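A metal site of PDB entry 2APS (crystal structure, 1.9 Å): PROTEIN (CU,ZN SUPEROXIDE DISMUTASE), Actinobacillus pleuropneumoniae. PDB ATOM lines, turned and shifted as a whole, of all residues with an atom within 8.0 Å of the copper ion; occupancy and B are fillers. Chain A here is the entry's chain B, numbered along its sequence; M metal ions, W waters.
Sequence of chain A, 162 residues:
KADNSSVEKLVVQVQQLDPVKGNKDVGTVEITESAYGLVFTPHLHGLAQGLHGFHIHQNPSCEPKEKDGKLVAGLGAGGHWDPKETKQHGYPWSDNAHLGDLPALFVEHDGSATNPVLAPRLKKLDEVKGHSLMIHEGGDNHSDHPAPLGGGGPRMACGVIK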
ATOM      1  N   GLY A  53     -19.657  -3.966  15.855  1.00  0.00           N
ATOM      2  CA  GLY A  53     -18.907  -5.171  16.172  1.00  0.00           C
ATOM      3  C   GLY A  53     -19.910  -6.313  16.278  1.00  0.00           C
ATOM      4  O   GLY A  53     -20.949  -6.163  16.907  1.00  0.00           O
ATOM      5  N   PHE A  54     -19.551  -7.447  15.687  1.00  0.00           N
ATOM      6  CA  PHE A  54     -20.404  -8.628  15.618  1.00  0.00           C
ATOM      7  C   PHE A  54     -19.596  -9.869  16.007  1.00  0.00           C
ATOM      8  O   PHE A  54     -18.731 -10.307  15.247  1.00  0.00           O
ATOM      9  CB  PHE A  54     -20.879  -8.738  14.159  1.00  0.00           C
ATOM     10  CG  PHE A  54     -22.054  -9.650  13.925  1.00  0.00           C
ATOM     11  CD1 PHE A  54     -23.048  -9.816  14.894  1.00  0.00           C
ATOM     12  CD2 PHE A  54     -22.196 -10.306  12.701  1.00  0.00           C
ATOM     13  CE1 PHE A  54     -24.157 -10.603  14.639  1.00  0.00           C
ATOM     14  CE2 PHE A  54     -23.308 -11.108  12.440  1.00  0.00           C
ATOM     15  CZ  PHE A  54     -24.291 -11.252  13.413  1.00  0.00           C
ATOM     16  N   HIS A  55     -19.859 -10.436  17.187  1.00  0.00           N
ATOM     17  CA  HIS A  55     -19.117 -11.623  17.625  1.00  0.00           C
ATOM     18  C   HIS A  55     -19.951 -12.621  18.411  1.00  0.00           C
ATOM     19  O   HIS A  55     -20.999 -12.293  18.977  1.00  0.00           O
ATOM     20  CB  HIS A  55     -17.917 -11.279  18.514  1.00  0.00           C
ATOM     21  CG  HIS A  55     -17.467  -9.855  18.433  1.00  0.00           C
ATOM     22  ND1 HIS A  55     -17.827  -8.906  19.365  1.00  0.00           N
ATOM     23  CD2 HIS A  55     -16.671  -9.214  17.543  1.00  0.00           C
ATOM     24  CE1 HIS A  55     -17.271  -7.750  19.055  1.00  0.00           C
ATOM     25  NE2 HIS A  55     -16.564  -7.910  17.955  1.00  0.00           N
ATOM     26  N   ILE A  56     -19.408 -13.829  18.508  1.00  0.00           N
ATOM     27  CA  ILE A  56     -20.034 -14.898  19.251  1.00  0.00           C
ATOM     28  C   ILE A  56     -19.349 -14.861  20.617  1.00  0.00           C
ATOM     29  O   ILE A  56     -18.128 -14.742  20.685  1.00  0.00           O
ATOM     30  CB  ILE A  56     -19.785 -16.242  18.559  1.00  0.00           C
ATOM     31  CG1 ILE A  56     -20.557 -16.266  17.242  1.00  0.00           C
ATOM     32  CG2 ILE A  56     -20.165 -17.410  19.465  1.00  0.00           C
ATOM     33  CD1 ILE A  56     -20.369 -17.526  16.460  1.00  0.00           C
ATOM     34  N   HIS A  57     -20.132 -14.815  21.685  1.00  0.00           N
ATOM     35  CA  HIS A  57     -19.580 -14.795  23.028  1.00  0.00           C
ATOM     36  C   HIS A  57     -19.727 -16.161  23.667  1.00  0.00           C
ATOM     37  O   HIS A  57     -20.505 -17.002  23.198  1.00  0.00           O
ATOM     38  CB  HIS A  57     -20.238 -13.706  23.868  1.00  0.00           C
ATOM     39  CG  HIS A  57     -19.760 -12.320  23.534  1.00  0.00           C
ATOM     40  ND1 HIS A  57     -19.296 -11.439  24.483  1.00  0.00           N
ATOM     41  CD2 HIS A  57     -19.633 -11.695  22.339  1.00  0.00           C
ATOM     42  CE1 HIS A  57     -18.902 -10.334  23.894  1.00  0.00           C
ATOM     43  NE2 HIS A  57     -19.099 -10.454  22.588  1.00  0.00           N
ATOM     44  N   ALA A  77     -23.195 -12.795  28.998  1.00  0.00           N
ATOM     45  CA  ALA A  77     -22.709 -13.515  27.834  1.00  0.00           C
ATOM     46  C   ALA A  77     -21.233 -13.893  27.933  1.00  0.00           C
ATOM     47  O   ALA A  77     -20.747 -14.739  27.191  1.00  0.00           O
ATOM     48  CB  ALA A  77     -22.966 -12.712  26.570  1.00  0.00           C
ATOM     49  N   GLY A  78     -20.515 -13.285  28.871  1.00  0.00           N
ATOM     50  CA  GLY A  78     -19.095 -13.577  29.001  1.00  0.00           C
ATOM     51  C   GLY A  78     -18.292 -12.897  27.909  1.00  0.00           C
ATOM     52  O   GLY A  78     -18.781 -11.993  27.227  1.00  0.00           O
ATOM     53  N   GLY A  79     -17.045 -13.341  27.720  1.00  0.00           N
ATOM     54  CA  GLY A  79     -16.194 -12.731  26.707  1.00  0.00           C
ATOM     55  C   GLY A  79     -16.340 -13.378  25.339  1.00  0.00           C
ATOM     56  O   GLY A  79     -17.216 -14.220  25.138  1.00  0.00           O
ATOM     57  N   HIS A  80     -15.471 -13.002  24.408  1.00  0.00           N
ATOM     58  CA  HIS A  80     -15.517 -13.555  23.061  1.00  0.00           C
ATOM     59  C   HIS A  80     -15.220 -15.049  23.108  1.00  0.00           C
ATOM     60  O   HIS A  80     -14.405 -15.508  23.924  1.00  0.00           O
ATOM     61  CB  HIS A  80     -14.521 -12.849  22.147  1.00  0.00           C
ATOM     62  CG  HIS A  80     -14.830 -11.409  21.897  1.00  0.00           C
ATOM     63  ND1 HIS A  80     -14.224 -10.672  20.900  1.00  0.00           N
ATOM     64  CD2 HIS A  80     -15.701 -10.559  22.499  1.00  0.00           C
ATOM     65  CE1 HIS A  80     -14.713  -9.451  20.896  1.00  0.00           C
ATOM     66  NE2 HIS A  80     -15.614  -9.354  21.856  1.00  0.00           N
ATOM     67  N   TRP A  81     -15.921 -15.811  22.278  1.00  0.00           N
ATOM     68  CA  TRP A  81     -15.737 -17.264  22.207  1.00  0.00           C
ATOM     69  C   TRP A  81     -14.333 -17.505  21.633  1.00  0.00           C
ATOM     70  O   TRP A  81     -14.039 -17.113  20.502  1.00  0.00           O
ATOM     71  CB  TRP A  81     -16.828 -17.854  21.310  1.00  0.00           C
ATOM     72  CG  TRP A  81     -16.788 -19.322  21.187  1.00  0.00           C
ATOM     73  CD1 TRP A  81     -16.535 -20.228  22.184  1.00  0.00           C
ATOM     74  CD2 TRP A  81     -16.984 -20.081  19.989  1.00  0.00           C
ATOM     75  NE1 TRP A  81     -16.583 -21.509  21.669  1.00  0.00           N
ATOM     76  CE2 TRP A  81     -16.864 -21.444  20.329  1.00  0.00           C
ATOM     77  CE3 TRP A  81     -17.269 -19.738  18.659  1.00  0.00           C
ATOM     78  CZ2 TRP A  81     -17.010 -22.470  19.389  1.00  0.00           C
ATOM     79  CZ3 TRP A  81     -17.420 -20.757  17.719  1.00  0.00           C
ATOM     80  CH2 TRP A  81     -17.288 -22.106  18.095  1.00  0.00           C
ATOM     81  N   HIS A  89      -7.965 -10.545  19.781  1.00  0.00           N
ATOM     82  CA  HIS A  89      -9.099 -10.197  18.941  1.00  0.00           C
ATOM     83  C   HIS A  89      -8.520  -9.859  17.570  1.00  0.00           C
ATOM     84  O   HIS A  89      -7.585  -9.062  17.475  1.00  0.00           O
ATOM     85  CB  HIS A  89      -9.852  -8.979  19.492  1.00  0.00           C
ATOM     86  CG  HIS A  89     -11.058  -8.608  18.687  1.00  0.00           C
ATOM     87  ND1 HIS A  89     -12.191  -9.395  18.640  1.00  0.00           N
ATOM     88  CD2 HIS A  89     -11.279  -7.575  17.836  1.00  0.00           C
ATOM     89  CE1 HIS A  89     -13.062  -8.855  17.794  1.00  0.00           C
ATOM     90  NE2 HIS A  89     -12.525  -7.757  17.291  1.00  0.00           N
ATOM     91  N   HIS A  98      -9.934 -14.746  17.905  1.00  0.00           N
ATOM     92  CA  HIS A  98     -10.943 -15.558  18.606  1.00  0.00           C
ATOM     93  C   HIS A  98     -11.818 -16.213  17.521  1.00  0.00           C
ATOM     94  O   HIS A  98     -12.188 -15.548  16.551  1.00  0.00           O
ATOM     95  CB  HIS A  98     -11.873 -14.679  19.466  1.00  0.00           C
ATOM     96  CG  HIS A  98     -11.176 -13.779  20.434  1.00  0.00           C
ATOM     97  ND1 HIS A  98     -11.479 -12.441  20.551  1.00  0.00           N
ATOM     98  CD2 HIS A  98     -10.227 -14.034  21.372  1.00  0.00           C
ATOM     99  CE1 HIS A  98     -10.761 -11.906  21.523  1.00  0.00           C
ATOM    100  NE2 HIS A  98      -9.992 -12.848  22.036  1.00  0.00           N
ATOM    101  N   GLY A 100     -14.841 -16.719  17.617  1.00  0.00           N
ATOM    102  CA  GLY A 100     -16.115 -16.001  17.564  1.00  0.00           C
ATOM    103  C   GLY A 100     -16.078 -14.650  16.860  1.00  0.00           C
ATOM    104  O   GLY A 100     -17.089 -13.956  16.811  1.00  0.00           O
ATOM    105  N   ASP A 101     -14.929 -14.264  16.293  1.00  0.00           N
ATOM    106  CA  ASP A 101     -14.792 -12.974  15.598  1.00  0.00           C
ATOM    107  C   ASP A 101     -15.385 -12.994  14.188  1.00  0.00           C
ATOM    108  O   ASP A 101     -14.824 -13.594  13.269  1.00  0.00           O
ATOM    109  CB  ASP A 101     -13.310 -12.548  15.547  1.00  0.00           C
ATOM    110  CG  ASP A 101     -12.739 -12.217  16.933  1.00  0.00           C
ATOM    111  OD1 ASP A 101     -13.527 -12.031  17.894  1.00  0.00           O
ATOM    112  OD2 ASP A 101     -11.512 -12.138  17.059  1.00  0.00           O
ATOM    113  N   SER A 132     -23.625 -17.233  22.538  1.00  0.00           N
ATOM    114  CA  SER A 132     -24.432 -16.057  22.264  1.00  0.00           C
ATOM    115  C   SER A 132     -23.864 -15.223  21.110  1.00  0.00           C
ATOM    116  O   SER A 132     -22.664 -15.267  20.821  1.00  0.00           O
ATOM    117  CB  SER A 132     -24.595 -15.202  23.538  1.00  0.00           C
ATOM    118  OG  SER A 132     -23.349 -14.889  24.120  1.00  0.00           O
ATOM    119  N   LEU A 133     -24.765 -14.528  20.403  1.00  0.00           N
ATOM    120  CA  LEU A 133     -24.421 -13.677  19.273  1.00  0.00           C
ATOM    121  C   LEU A 133     -24.576 -12.241  19.753  1.00  0.00           C
ATOM    122  O   LEU A 133     -25.674 -11.818  20.113  1.00  0.00           O
ATOM    123  CB  LEU A 133     -25.385 -13.950  18.118  1.00  0.00           C
ATOM    124  CG  LEU A 133     -25.135 -13.268  16.774  1.00  0.00           C
ATOM    125  CD1 LEU A 133     -23.751 -13.675  16.233  1.00  0.00           C
ATOM    126  CD2 LEU A 133     -26.239 -13.685  15.795  1.00  0.00           C
ATOM    127  N   MET A 134     -23.475 -11.497  19.750  1.00  0.00           N
ATOM    128  CA  MET A 134     -23.467 -10.134  20.255  1.00  0.00           C
ATOM    129  C   MET A 134     -23.284  -9.046  19.193  1.00  0.00           C
ATOM    130  O   MET A 134     -22.482  -9.193  18.254  1.00  0.00           O
ATOM    131  CB  MET A 134     -22.347 -10.004  21.296  1.00  0.00           C
ATOM    132  CG  MET A 134     -22.392  -8.763  22.177  1.00  0.00           C
ATOM    133  SD  MET A 134     -23.787  -8.833  23.309  1.00  0.00           S
ATOM    134  CE  MET A 134     -23.307 -10.232  24.340  1.00  0.00           C
ATOM    135  N   ILE A 135     -24.051  -7.965  19.340  1.00  0.00           N
ATOM    136  CA  ILE A 135     -23.942  -6.804  18.457  1.00  0.00           C
ATOM    137  C   ILE A 135     -23.605  -5.630  19.378  1.00  0.00           C
ATOM    138  O   ILE A 135     -24.355  -5.315  20.320  1.00  0.00           O
ATOM    139  CB  ILE A 135     -25.250  -6.509  17.679  1.00  0.00           C
ATOM    140  CG1 ILE A 135     -25.663  -7.756  16.893  1.00  0.00           C
ATOM    141  CG2 ILE A 135     -25.009  -5.329  16.715  1.00  0.00           C
ATOM    142  CD1 ILE A 135     -27.006  -7.632  16.222  1.00  0.00           C
ATOM    143  N   HIS A 136     -22.460  -5.003  19.105  1.00  0.00           N
ATOM    144  CA  HIS A 136     -21.985  -3.897  19.919  1.00  0.00           C
ATOM    145  C   HIS A 136     -22.393  -2.514  19.466  1.00  0.00           C
ATOM    146  O   HIS A 136     -22.779  -2.299  18.305  1.00  0.00           O
ATOM    147  CB  HIS A 136     -20.466  -3.934  20.041  1.00  0.00           C
ATOM    148  CG  HIS A 136     -19.969  -5.131  20.787  1.00  0.00           C
ATOM    149  ND1 HIS A 136     -19.607  -5.070  22.114  1.00  0.00           N
ATOM    150  CD2 HIS A 136     -19.841  -6.425  20.417  1.00  0.00           C
ATOM    151  CE1 HIS A 136     -19.287  -6.283  22.526  1.00  0.00           C
ATOM    152  NE2 HIS A 136     -19.412  -7.122  21.518  1.00  0.00           N
ATOM    153  N   ASP A 140     -15.582  -2.186  14.886  1.00  0.00           N
ATOM    154  CA  ASP A 140     -14.623  -3.268  15.033  1.00  0.00           C
ATOM    155  C   ASP A 140     -13.461  -3.125  14.059  1.00  0.00           C
ATOM    156  O   ASP A 140     -13.604  -3.347  12.857  1.00  0.00           O
ATOM    157  CB  ASP A 140     -15.327  -4.613  14.813  1.00  0.00           C
ATOM    158  CG  ASP A 140     -14.520  -5.793  15.323  1.00  0.00           C
ATOM    159  OD1 ASP A 140     -13.304  -5.634  15.589  1.00  0.00           O
ATOM    160  OD2 ASP A 140     -15.102  -6.882  15.482  1.00  0.00           O
ATOM    161  N   LEU A 149     -10.666  -5.494  22.273  1.00  0.00           N
ATOM    162  CA  LEU A 149     -11.727  -6.174  21.532  1.00  0.00           C
ATOM    163  C   LEU A 149     -12.295  -5.391  20.339  1.00  0.00           C
ATOM    164  O   LEU A 149     -13.513  -5.382  20.114  1.00  0.00           O
ATOM    165  CB  LEU A 149     -12.850  -6.592  22.501  1.00  0.00           C
ATOM    166  CG  LEU A 149     -12.405  -7.472  23.675  1.00  0.00           C
ATOM    167  CD1 LEU A 149     -13.526  -7.645  24.670  1.00  0.00           C
ATOM    168  CD2 LEU A 149     -11.889  -8.832  23.179  1.00  0.00           C
ATOM    169  N   GLY A 152     -15.461  -2.331  20.315  1.00  0.00           N
ATOM    170  CA  GLY A 152     -16.905  -2.526  20.349  1.00  0.00           C
ATOM    171  C   GLY A 152     -17.654  -1.824  21.486  1.00  0.00           C
ATOM    172  O   GLY A 152     -18.785  -1.386  21.315  1.00  0.00           O
ATOM    173  N   GLY A 153     -17.025  -1.747  22.656  1.00  0.00           N
ATOM    174  CA  GLY A 153     -17.682  -1.101  23.783  1.00  0.00           C
ATOM    175  C   GLY A 153     -18.926  -1.810  24.277  1.00  0.00           C
ATOM    176  O   GLY A 153     -19.028  -3.042  24.189  1.00  0.00           O
ATOM    177  N   PRO A 154     -19.939  -1.057  24.740  1.00  0.00           N
ATOM    178  CA  PRO A 154     -21.212  -1.584  25.256  1.00  0.00           C
ATOM    179  C   PRO A 154     -21.898  -2.596  24.347  1.00  0.00           C
ATOM    180  O   PRO A 154     -21.705  -2.608  23.128  1.00  0.00           O
ATOM    181  CB  PRO A 154     -22.059  -0.322  25.421  1.00  0.00           C
ATOM    182  CG  PRO A 154     -21.038   0.731  25.718  1.00  0.00           C
ATOM    183  CD  PRO A 154     -19.948   0.422  24.724  1.00  0.00           C
ATOM    184  N   ARG A 155     -22.730  -3.417  24.967  1.00  0.00           N
ATOM    185  CA  ARG A 155     -23.471  -4.454  24.264  1.00  0.00           C
ATOM    186  C   ARG A 155     -24.848  -3.920  23.920  1.00  0.00           C
ATOM    187  O   ARG A 155     -25.650  -3.625  24.801  1.00  0.00           O
ATOM    188  CB  ARG A 155     -23.505  -5.696  25.153  1.00  0.00           C
ATOM    189  CG  ARG A 155     -22.083  -6.194  25.382  1.00  0.00           C
ATOM    190  CD  ARG A 155     -21.935  -7.237  26.469  1.00  0.00           C
ATOM    191  NE  ARG A 155     -20.517  -7.538  26.662  1.00  0.00           N
ATOM    192  CZ  ARG A 155     -20.047  -8.691  27.137  1.00  0.00           C
ATOM    193  NH1 ARG A 155     -20.877  -9.665  27.467  1.00  0.00           N
ATOM    194  NH2 ARG A 155     -18.738  -8.854  27.267  1.00  0.00           N
HETATM  195 CU    CU M   1     -18.526  -9.039  21.224  1.00  0.00          CU
HETATM  196 ZN    ZN M   2     -12.743 -11.229  19.556  1.00  0.00          ZN
HETATM  197  O   HOH W   1     -17.011  -8.006  23.760  1.00  0.00           O
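Residues that only touch the copper ion: His 80 and Met 134.
Five residues have an atom within 4 Å of the copper ion: His 55, His 57, His 80, Met 134 and His 136.
The nearest printed residue that does not touch the copper ion is Phe 54 (5.4 Å).
The copper ion is bound by a ring nitrogen (ND1) of His 55 (2.0 Å), a ring nitrogen (NE2) of His 57 (2.0 Å) and a ring nitrogen (NE2) of His 136 (2.1 Å).
The copper ion has three donor atoms within binding distance.
The backbone NH of His 136 lies within hydrogen-bond range of the backbone carbonyl oxygen of Gly 53.
N of His 57 is in hydrogen-bond range of O of Ser 132 (2.7 Å).
OD2 of Asp 140 is in hydrogen-bond range of NE2 of His 55, 3.1 Å away.
A ring nitrogen (ND1) of His 136 is in hydrogen-bond range of the backbone carbonyl oxygen of Pro 154.
O of Gly 78 is in hydrogen-bond range of ND1 of His 57 (2.8 Å).
The backbone carbonyl oxygen (O) of His 55 sits at hydrogen-bond distance from the backbone NH (N) of Met 134, at 2.7 Å.
A ring nitrogen (NE2) of His 80 lies close to a ring nitrogen (ND1) of His 55, 3.4 Å away.
ND1 of His 136 is in hydrogen-bond range of O of Gly 153.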
